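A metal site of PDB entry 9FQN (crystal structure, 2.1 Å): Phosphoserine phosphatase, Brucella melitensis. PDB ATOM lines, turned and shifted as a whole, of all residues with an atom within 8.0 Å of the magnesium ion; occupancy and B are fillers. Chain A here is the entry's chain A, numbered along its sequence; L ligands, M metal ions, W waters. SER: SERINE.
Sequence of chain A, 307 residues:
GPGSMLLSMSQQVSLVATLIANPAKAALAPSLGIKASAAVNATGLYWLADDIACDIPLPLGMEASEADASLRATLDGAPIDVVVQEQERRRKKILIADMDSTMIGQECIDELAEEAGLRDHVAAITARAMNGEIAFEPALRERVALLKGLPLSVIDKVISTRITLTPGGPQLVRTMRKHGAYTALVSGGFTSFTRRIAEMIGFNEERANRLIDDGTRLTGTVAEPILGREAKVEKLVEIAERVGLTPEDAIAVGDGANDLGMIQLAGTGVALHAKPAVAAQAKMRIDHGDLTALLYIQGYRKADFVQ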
ATOM      1  N   ALA A  97      17.346  22.386   3.023  1.00  0.00           N
ATOM      2  CA  ALA A  97      16.578  21.163   2.815  1.00  0.00           C
ATOM      3  C   ALA A  97      17.491  20.011   2.416  1.00  0.00           C
ATOM      4  O   ALA A  97      18.323  20.162   1.517  1.00  0.00           O
ATOM      5  CB  ALA A  97      15.518  21.374   1.731  1.00  0.00           C
ATOM      6  N   ASP A  98      17.334  18.876   3.072  1.00  0.00           N
ATOM      7  CA  ASP A  98      18.002  17.670   2.597  1.00  0.00           C
ATOM      8  C   ASP A  98      17.454  17.259   1.236  1.00  0.00           C
ATOM      9  O   ASP A  98      16.340  17.637   0.855  1.00  0.00           O
ATOM     10  CB  ASP A  98      17.815  16.544   3.611  1.00  0.00           C
ATOM     11  CG  ASP A  98      18.478  15.268   3.157  1.00  0.00           C
ATOM     12  OD1 ASP A  98      19.684  15.292   2.833  1.00  0.00           O
ATOM     13  OD2 ASP A  98      17.780  14.247   3.121  1.00  0.00           O
ATOM     14  N   MET A  99      18.230  16.477   0.482  1.00  0.00           N
ATOM     15  CA  MET A  99      17.774  16.014  -0.842  1.00  0.00           C
ATOM     16  C   MET A  99      17.146  14.624  -0.777  1.00  0.00           C
ATOM     17  O   MET A  99      15.951  14.476  -1.027  1.00  0.00           O
ATOM     18  CB  MET A  99      18.918  16.036  -1.861  1.00  0.00           C
ATOM     19  CG  MET A  99      18.553  15.278  -3.137  1.00  0.00           C
ATOM     20  SD  MET A  99      19.791  15.357  -4.447  1.00  0.00           S
ATOM     21  CE  MET A  99      20.650  13.832  -4.083  1.00  0.00           C
ATOM     22  N   ASP A 100      17.946  13.605  -0.443  1.00  0.00           N
ATOM     23  CA  ASP A 100      17.484  12.216  -0.522  1.00  0.00           C
ATOM     24  C   ASP A 100      16.239  12.009   0.324  1.00  0.00           C
ATOM     25  O   ASP A 100      16.220  12.324   1.519  1.00  0.00           O
ATOM     26  CB  ASP A 100      18.589  11.256  -0.074  1.00  0.00           C
ATOM     27  CG  ASP A 100      19.776  11.218  -1.014  1.00  0.00           C
ATOM     28  OD1 ASP A 100      19.613  10.935  -2.226  1.00  0.00           O
ATOM     29  OD2 ASP A 100      20.902  11.454  -0.548  1.00  0.00           O
ATOM     30  N   SER A 101      15.178  11.481  -0.299  1.00  0.00           N
ATOM     31  CA  SER A 101      13.911  11.166   0.350  1.00  0.00           C
ATOM     32  C   SER A 101      13.240  12.386   0.951  1.00  0.00           C
ATOM     33  O   SER A 101      12.317  12.249   1.742  1.00  0.00           O
ATOM     34  CB  SER A 101      14.081  10.078   1.428  1.00  0.00           C
ATOM     35  OG  SER A 101      14.552   8.868   0.840  1.00  0.00           O
ATOM     36  N   THR A 102      13.709  13.588   0.606  1.00  0.00           N
ATOM     37  CA  THR A 102      13.069  14.820   1.050  1.00  0.00           C
ATOM     38  C   THR A 102      12.627  15.602  -0.179  1.00  0.00           C
ATOM     39  O   THR A 102      11.425  15.621  -0.474  1.00  0.00           O
ATOM     40  CB  THR A 102      13.999  15.608   1.990  1.00  0.00           C
ATOM     41  OG1 THR A 102      14.300  14.811   3.141  1.00  0.00           O
ATOM     42  CG2 THR A 102      13.338  16.883   2.467  1.00  0.00           C
ATOM     43  N   MET A 103      13.552  16.166  -0.956  1.00  0.00           N
ATOM     44  CA  MET A 103      13.155  16.825  -2.200  1.00  0.00           C
ATOM     45  C   MET A 103      13.086  15.891  -3.378  1.00  0.00           C
ATOM     46  O   MET A 103      12.493  16.249  -4.399  1.00  0.00           O
ATOM     47  CB  MET A 103      14.093  18.001  -2.514  1.00  0.00           C
ATOM     48  CG  MET A 103      14.431  18.796  -1.281  1.00  0.00           C
ATOM     49  SD  MET A 103      13.080  19.874  -0.751  1.00  0.00           S
ATOM     50  CE  MET A 103      12.553  20.456  -2.367  1.00  0.00           C
ATOM     51  N   ILE A 104      13.686  14.706  -3.283  1.00  0.00           N
ATOM     52  CA  ILE A 104      13.502  13.682  -4.301  1.00  0.00           C
ATOM     53  C   ILE A 104      12.909  12.467  -3.624  1.00  0.00           C
ATOM     54  O   ILE A 104      12.971  12.318  -2.393  1.00  0.00           O
ATOM     55  CB  ILE A 104      14.800  13.330  -5.038  1.00  0.00           C
ATOM     56  CG1 ILE A 104      15.879  12.862  -4.043  1.00  0.00           C
ATOM     57  CG2 ILE A 104      15.302  14.519  -5.827  1.00  0.00           C
ATOM     58  CD1 ILE A 104      17.042  12.182  -4.748  1.00  0.00           C
ATOM     59  N   GLN A 106      13.839   9.402  -3.917  1.00  0.00           N
ATOM     60  CA  GLN A 106      14.791   8.298  -3.868  1.00  0.00           C
ATOM     61  C   GLN A 106      15.981   8.617  -2.965  1.00  0.00           C
ATOM     62  O   GLN A 106      16.187   9.744  -2.501  1.00  0.00           O
ATOM     63  CB  GLN A 106      15.283   7.958  -5.274  1.00  0.00           C
ATOM     64  CG  GLN A 106      14.208   7.537  -6.281  1.00  0.00           C
ATOM     65  CD  GLN A 106      13.305   8.676  -6.706  1.00  0.00           C
ATOM     66  OE1 GLN A 106      13.740   9.826  -6.821  1.00  0.00           O
ATOM     67  NE2 GLN A 106      12.029   8.369  -6.939  1.00  0.00           N
ATOM     68  N   GLU A 107      16.762   7.575  -2.700  1.00  0.00           N
ATOM     69  CA  GLU A 107      18.091   7.684  -2.103  1.00  0.00           C
ATOM     70  C   GLU A 107      19.087   7.531  -3.250  1.00  0.00           C
ATOM     71  O   GLU A 107      19.193   6.439  -3.821  1.00  0.00           O
ATOM     72  CB  GLU A 107      18.293   6.594  -1.042  1.00  0.00           C
ATOM     73  CG  GLU A 107      17.465   6.761   0.221  1.00  0.00           C
ATOM     74  CD  GLU A 107      17.997   7.855   1.110  1.00  0.00           C
ATOM     75  OE1 GLU A 107      19.214   8.151   1.007  1.00  0.00           O
ATOM     76  OE2 GLU A 107      17.229   8.426   1.897  1.00  0.00           O
ATOM     77  N   THR A 126      21.582   1.955   4.146  1.00  0.00           N
ATOM     78  CA  THR A 126      21.005   3.295   4.095  1.00  0.00           C
ATOM     79  C   THR A 126      19.905   3.462   5.121  1.00  0.00           C
ATOM     80  O   THR A 126      19.857   4.462   5.841  1.00  0.00           O
ATOM     81  CB  THR A 126      20.468   3.573   2.696  1.00  0.00           C
ATOM     82  OG1 THR A 126      21.532   3.405   1.754  1.00  0.00           O
ATOM     83  CG2 THR A 126      19.953   4.975   2.591  1.00  0.00           C
ATOM     84  N   MET A 130      19.966   6.066   8.080  1.00  0.00           N
ATOM     85  CA  MET A 130      18.989   7.130   8.200  1.00  0.00           C
ATOM     86  C   MET A 130      18.166   7.028   9.488  1.00  0.00           C
ATOM     87  O   MET A 130      17.676   8.061   9.967  1.00  0.00           O
ATOM     88  CB  MET A 130      18.105   7.157   6.958  1.00  0.00           C
ATOM     89  CG  MET A 130      18.887   7.622   5.687  1.00  0.00           C
ATOM     90  SD  MET A 130      19.568   9.309   5.725  1.00  0.00           S
ATOM     91  CE  MET A 130      21.223   9.090   6.439  1.00  0.00           C
ATOM     92  N   VAL A 186      21.148  20.929   0.873  1.00  0.00           N
ATOM     93  CA  VAL A 186      22.323  20.306   1.475  1.00  0.00           C
ATOM     94  C   VAL A 186      22.051  18.820   1.644  1.00  0.00           C
ATOM     95  O   VAL A 186      20.919  18.408   1.912  1.00  0.00           O
ATOM     96  CB  VAL A 186      22.692  20.967   2.808  1.00  0.00           C
ATOM     97  CG1 VAL A 186      22.716  22.463   2.633  1.00  0.00           C
ATOM     98  CG2 VAL A 186      21.702  20.542   3.888  1.00  0.00           C
ATOM     99  N   SER A 187      23.085  18.006   1.439  1.00  0.00           N
ATOM    100  CA  SER A 187      22.881  16.585   1.244  1.00  0.00           C
ATOM    101  C   SER A 187      24.119  15.814   1.668  1.00  0.00           C
ATOM    102  O   SER A 187      25.231  16.231   1.361  1.00  0.00           O
ATOM    103  CB  SER A 187      22.536  16.302  -0.237  1.00  0.00           C
ATOM    104  OG  SER A 187      22.562  14.921  -0.530  1.00  0.00           O
ATOM    105  N   GLY A 188      23.921  14.705   2.395  1.00  0.00           N
ATOM    106  CA  GLY A 188      24.979  13.715   2.507  1.00  0.00           C
ATOM    107  C   GLY A 188      25.225  12.919   1.242  1.00  0.00           C
ATOM    108  O   GLY A 188      26.146  12.098   1.202  1.00  0.00           O
ATOM    109  N   GLY A 189      24.416  13.146   0.207  1.00  0.00           N
ATOM    110  CA  GLY A 189      24.610  12.501  -1.078  1.00  0.00           C
ATOM    111  C   GLY A 189      25.641  13.238  -1.898  1.00  0.00           C
ATOM    112  O   GLY A 189      26.580  13.839  -1.358  1.00  0.00           O
ATOM    113  N   LYS A 232      25.903  19.800   8.075  1.00  0.00           N
ATOM    114  CA  LYS A 232      24.646  20.494   7.794  1.00  0.00           C
ATOM    115  C   LYS A 232      24.425  21.615   8.791  1.00  0.00           C
ATOM    116  O   LYS A 232      23.977  22.715   8.412  1.00  0.00           O
ATOM    117  CB  LYS A 232      23.456  19.499   7.824  1.00  0.00           C
ATOM    118  CG  LYS A 232      23.585  18.353   6.816  1.00  0.00           C
ATOM    119  CD  LYS A 232      22.316  17.487   6.697  1.00  0.00           C
ATOM    120  CE  LYS A 232      22.199  16.898   5.299  1.00  0.00           C
ATOM    121  NZ  LYS A 232      21.508  15.574   5.248  1.00  0.00           N
ATOM    122  N   VAL A 253      14.528  21.167   6.815  1.00  0.00           N
ATOM    123  CA  VAL A 253      13.651  20.012   6.594  1.00  0.00           C
ATOM    124  C   VAL A 253      14.481  18.814   6.160  1.00  0.00           C
ATOM    125  O   VAL A 253      15.315  18.900   5.258  1.00  0.00           O
ATOM    126  CB  VAL A 253      12.546  20.314   5.562  1.00  0.00           C
ATOM    127  CG1 VAL A 253      13.120  20.679   4.207  1.00  0.00           C
ATOM    128  CG2 VAL A 253      11.572  19.101   5.421  1.00  0.00           C
ATOM    129  N   GLY A 254      14.243  17.680   6.816  1.00  0.00           N
ATOM    130  CA  GLY A 254      14.856  16.437   6.384  1.00  0.00           C
ATOM    131  C   GLY A 254      14.086  15.260   6.931  1.00  0.00           C
ATOM    132  O   GLY A 254      13.053  15.414   7.596  1.00  0.00           O
ATOM    133  N   ASP A 255      14.584  14.063   6.618  1.00  0.00           N
ATOM    134  CA  ASP A 255      13.947  12.822   7.014  1.00  0.00           C
ATOM    135  C   ASP A 255      14.852  11.932   7.845  1.00  0.00           C
ATOM    136  O   ASP A 255      14.370  10.917   8.380  1.00  0.00           O
ATOM    137  CB  ASP A 255      13.491  12.032   5.784  1.00  0.00           C
ATOM    138  CG  ASP A 255      14.659  11.596   4.924  1.00  0.00           C
ATOM    139  OD1 ASP A 255      15.507  12.456   4.589  1.00  0.00           O
ATOM    140  OD2 ASP A 255      14.737  10.399   4.575  1.00  0.00           O
ATOM    141  N   GLY A 256      16.143  12.246   7.955  1.00  0.00           N
ATOM    142  CA  GLY A 256      17.131  11.317   8.450  1.00  0.00           C
ATOM    143  C   GLY A 256      17.755  11.804   9.742  1.00  0.00           C
ATOM    144  O   GLY A 256      17.583  12.960  10.174  1.00  0.00           O
ATOM    145  N   ALA A 257      18.491  10.883  10.377  1.00  0.00           N
ATOM    146  CA  ALA A 257      19.165  11.210  11.628  1.00  0.00           C
ATOM    147  C   ALA A 257      20.229  12.284  11.412  1.00  0.00           C
ATOM    148  O   ALA A 257      20.414  13.165  12.263  1.00  0.00           O
ATOM    149  CB  ALA A 257      19.793   9.937  12.221  1.00  0.00           C
ATOM    150  N   ASN A 258      20.902  12.257  10.274  1.00  0.00           N
ATOM    151  CA  ASN A 258      21.908  13.280  10.007  1.00  0.00           C
ATOM    152  C   ASN A 258      21.299  14.641   9.697  1.00  0.00           C
ATOM    153  O   ASN A 258      22.048  15.610   9.531  1.00  0.00           O
ATOM    154  CB  ASN A 258      22.845  12.826   8.880  1.00  0.00           C
ATOM    155  CG  ASN A 258      22.156  12.771   7.524  1.00  0.00           C
ATOM    156  OD1 ASN A 258      20.955  12.486   7.436  1.00  0.00           O
ATOM    157  ND2 ASN A 258      22.914  13.056   6.454  1.00  0.00           N
ATOM    158  N   ASP A 259      19.957  14.758   9.649  1.00  0.00           N
ATOM    159  CA  ASP A 259      19.309  16.056   9.485  1.00  0.00           C
ATOM    160  C   ASP A 259      18.910  16.683  10.806  1.00  0.00           C
ATOM    161  O   ASP A 259      18.532  17.849  10.828  1.00  0.00           O
ATOM    162  CB  ASP A 259      18.048  15.932   8.615  1.00  0.00           C
ATOM    163  CG  ASP A 259      18.355  15.432   7.224  1.00  0.00           C
ATOM    164  OD1 ASP A 259      19.300  15.976   6.604  1.00  0.00           O
ATOM    165  OD2 ASP A 259      17.680  14.500   6.751  1.00  0.00           O
ATOM    166  N   MET A 262      20.617  20.179  11.993  1.00  0.00           N
ATOM    167  CA  MET A 262      20.084  21.378  11.369  1.00  0.00           C
ATOM    168  C   MET A 262      18.609  21.587  11.692  1.00  0.00           C
ATOM    169  O   MET A 262      18.186  22.717  11.936  1.00  0.00           O
ATOM    170  CB  MET A 262      20.376  21.292   9.873  1.00  0.00           C
ATOM    171  CG  MET A 262      19.440  20.440   9.061  1.00  0.00           C
ATOM    172  SD  MET A 262      19.710  20.796   7.348  1.00  0.00           S
ATOM    173  CE  MET A 262      19.041  19.350   6.547  1.00  0.00           C
ATOM    174  N   LEU A 272      10.204  15.452   7.977  1.00  0.00           N
ATOM    175  CA  LEU A 272       9.257  15.235   6.883  1.00  0.00           C
ATOM    176  C   LEU A 272       9.240  13.755   6.530  1.00  0.00           C
ATOM    177  O   LEU A 272      10.238  13.227   6.033  1.00  0.00           O
ATOM    178  CB  LEU A 272       9.630  16.068   5.664  1.00  0.00           C
ATOM    179  CG  LEU A 272       8.713  15.875   4.463  1.00  0.00           C
ATOM    180  CD1 LEU A 272       7.349  16.455   4.764  1.00  0.00           C
ATOM    181  CD2 LEU A 272       9.324  16.517   3.263  1.00  0.00           C
HETATM  182  N   SER L   1      20.544   9.526   2.919  1.00  0.00           N
HETATM  183  CA  SER L   1      21.812   9.434   2.191  1.00  0.00           C
HETATM  184  C   SER L   1      22.747   8.370   2.764  1.00  0.00           C
HETATM  185  O   SER L   1      23.729   8.023   2.114  1.00  0.00           O
HETATM  186  CB  SER L   1      22.507  10.793   2.160  1.00  0.00           C
HETATM  187  OG  SER L   1      22.270  11.482   3.386  1.00  0.00           O
HETATM  188  OXT SER L   1      22.589   7.850   3.879  1.00  0.00           O
HETATM  189 MG    MG M   1      17.290  12.363   3.455  1.00  0.00          MG
HETATM  190  O   HOH W   1      17.427   9.926   3.629  1.00  0.00           O
HETATM  191  O   HOH W   2      19.474  12.029   3.063  1.00  0.00           O
HETATM  192  O   HOH W   3      19.172  12.720   5.655  1.00  0.00           O
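OD2 of Asp 100 lies within salt-bridge range of N of the ligand (3.98 Å). OE1 of Glu 107 lies within salt-bridge range of N of the ligand, 2.7 Å away. A nitrogen (N) of the ligand sits at hydrogen-bond distance from the side-chain sulfur (SD) of Met 130 (3.0 Å).
The side-chain amino group (NZ) of Lys 232 lies within salt-bridge range of the side-chain carboxylate (OD1) of Asp 98, at 3.0 Å. The backbone NH (N) of Asp 98 sits at hydrogen-bond distance from the backbone carbonyl oxygen (O) of Val 253 (3.0 Å). The side-chain hydroxyl of Thr 102 lies close to the side-chain carboxylate of Asp 255 (3.0 Å). N of Asp 255 sits at hydrogen-bond distance from OD2 of Asp 259 (3.1 Å). N of Gly 256 lies within hydrogen-bond range of OD2 of Asp 259 (3.0 Å). NZ of Lys 232 lies within salt-bridge range of OD1 of Asp 259, at 2.6 Å.
Thr 102 touches the magnesium ion (OG1 to MG, 3.9 Å). OD2 of Asp 259 touches the magnesium ion, 3.9 Å away.
The magnesium ion is bound by OD2 of Asp 98 (2.0 Å), OD1 of Asp 255 (2.1 Å), O of Asp 100 (2.2 Å), water W2 (2.2 Å) and water W1 (2.4 Å). The magnesium ion has five donor atoms within binding distance.
Water W2 bridges N of the ligand (2.7 Å) and OD1 of Asp 98 (3.3 Å). Water W1 lies within hydrogen-bond range of the side-chain carboxylate (OD2) of Asp 255 (2.9 Å), the side-chain sulfur (SD) of Met 130 (3.1 Å) and a nitrogen (N) of the ligand (3.2 Å).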
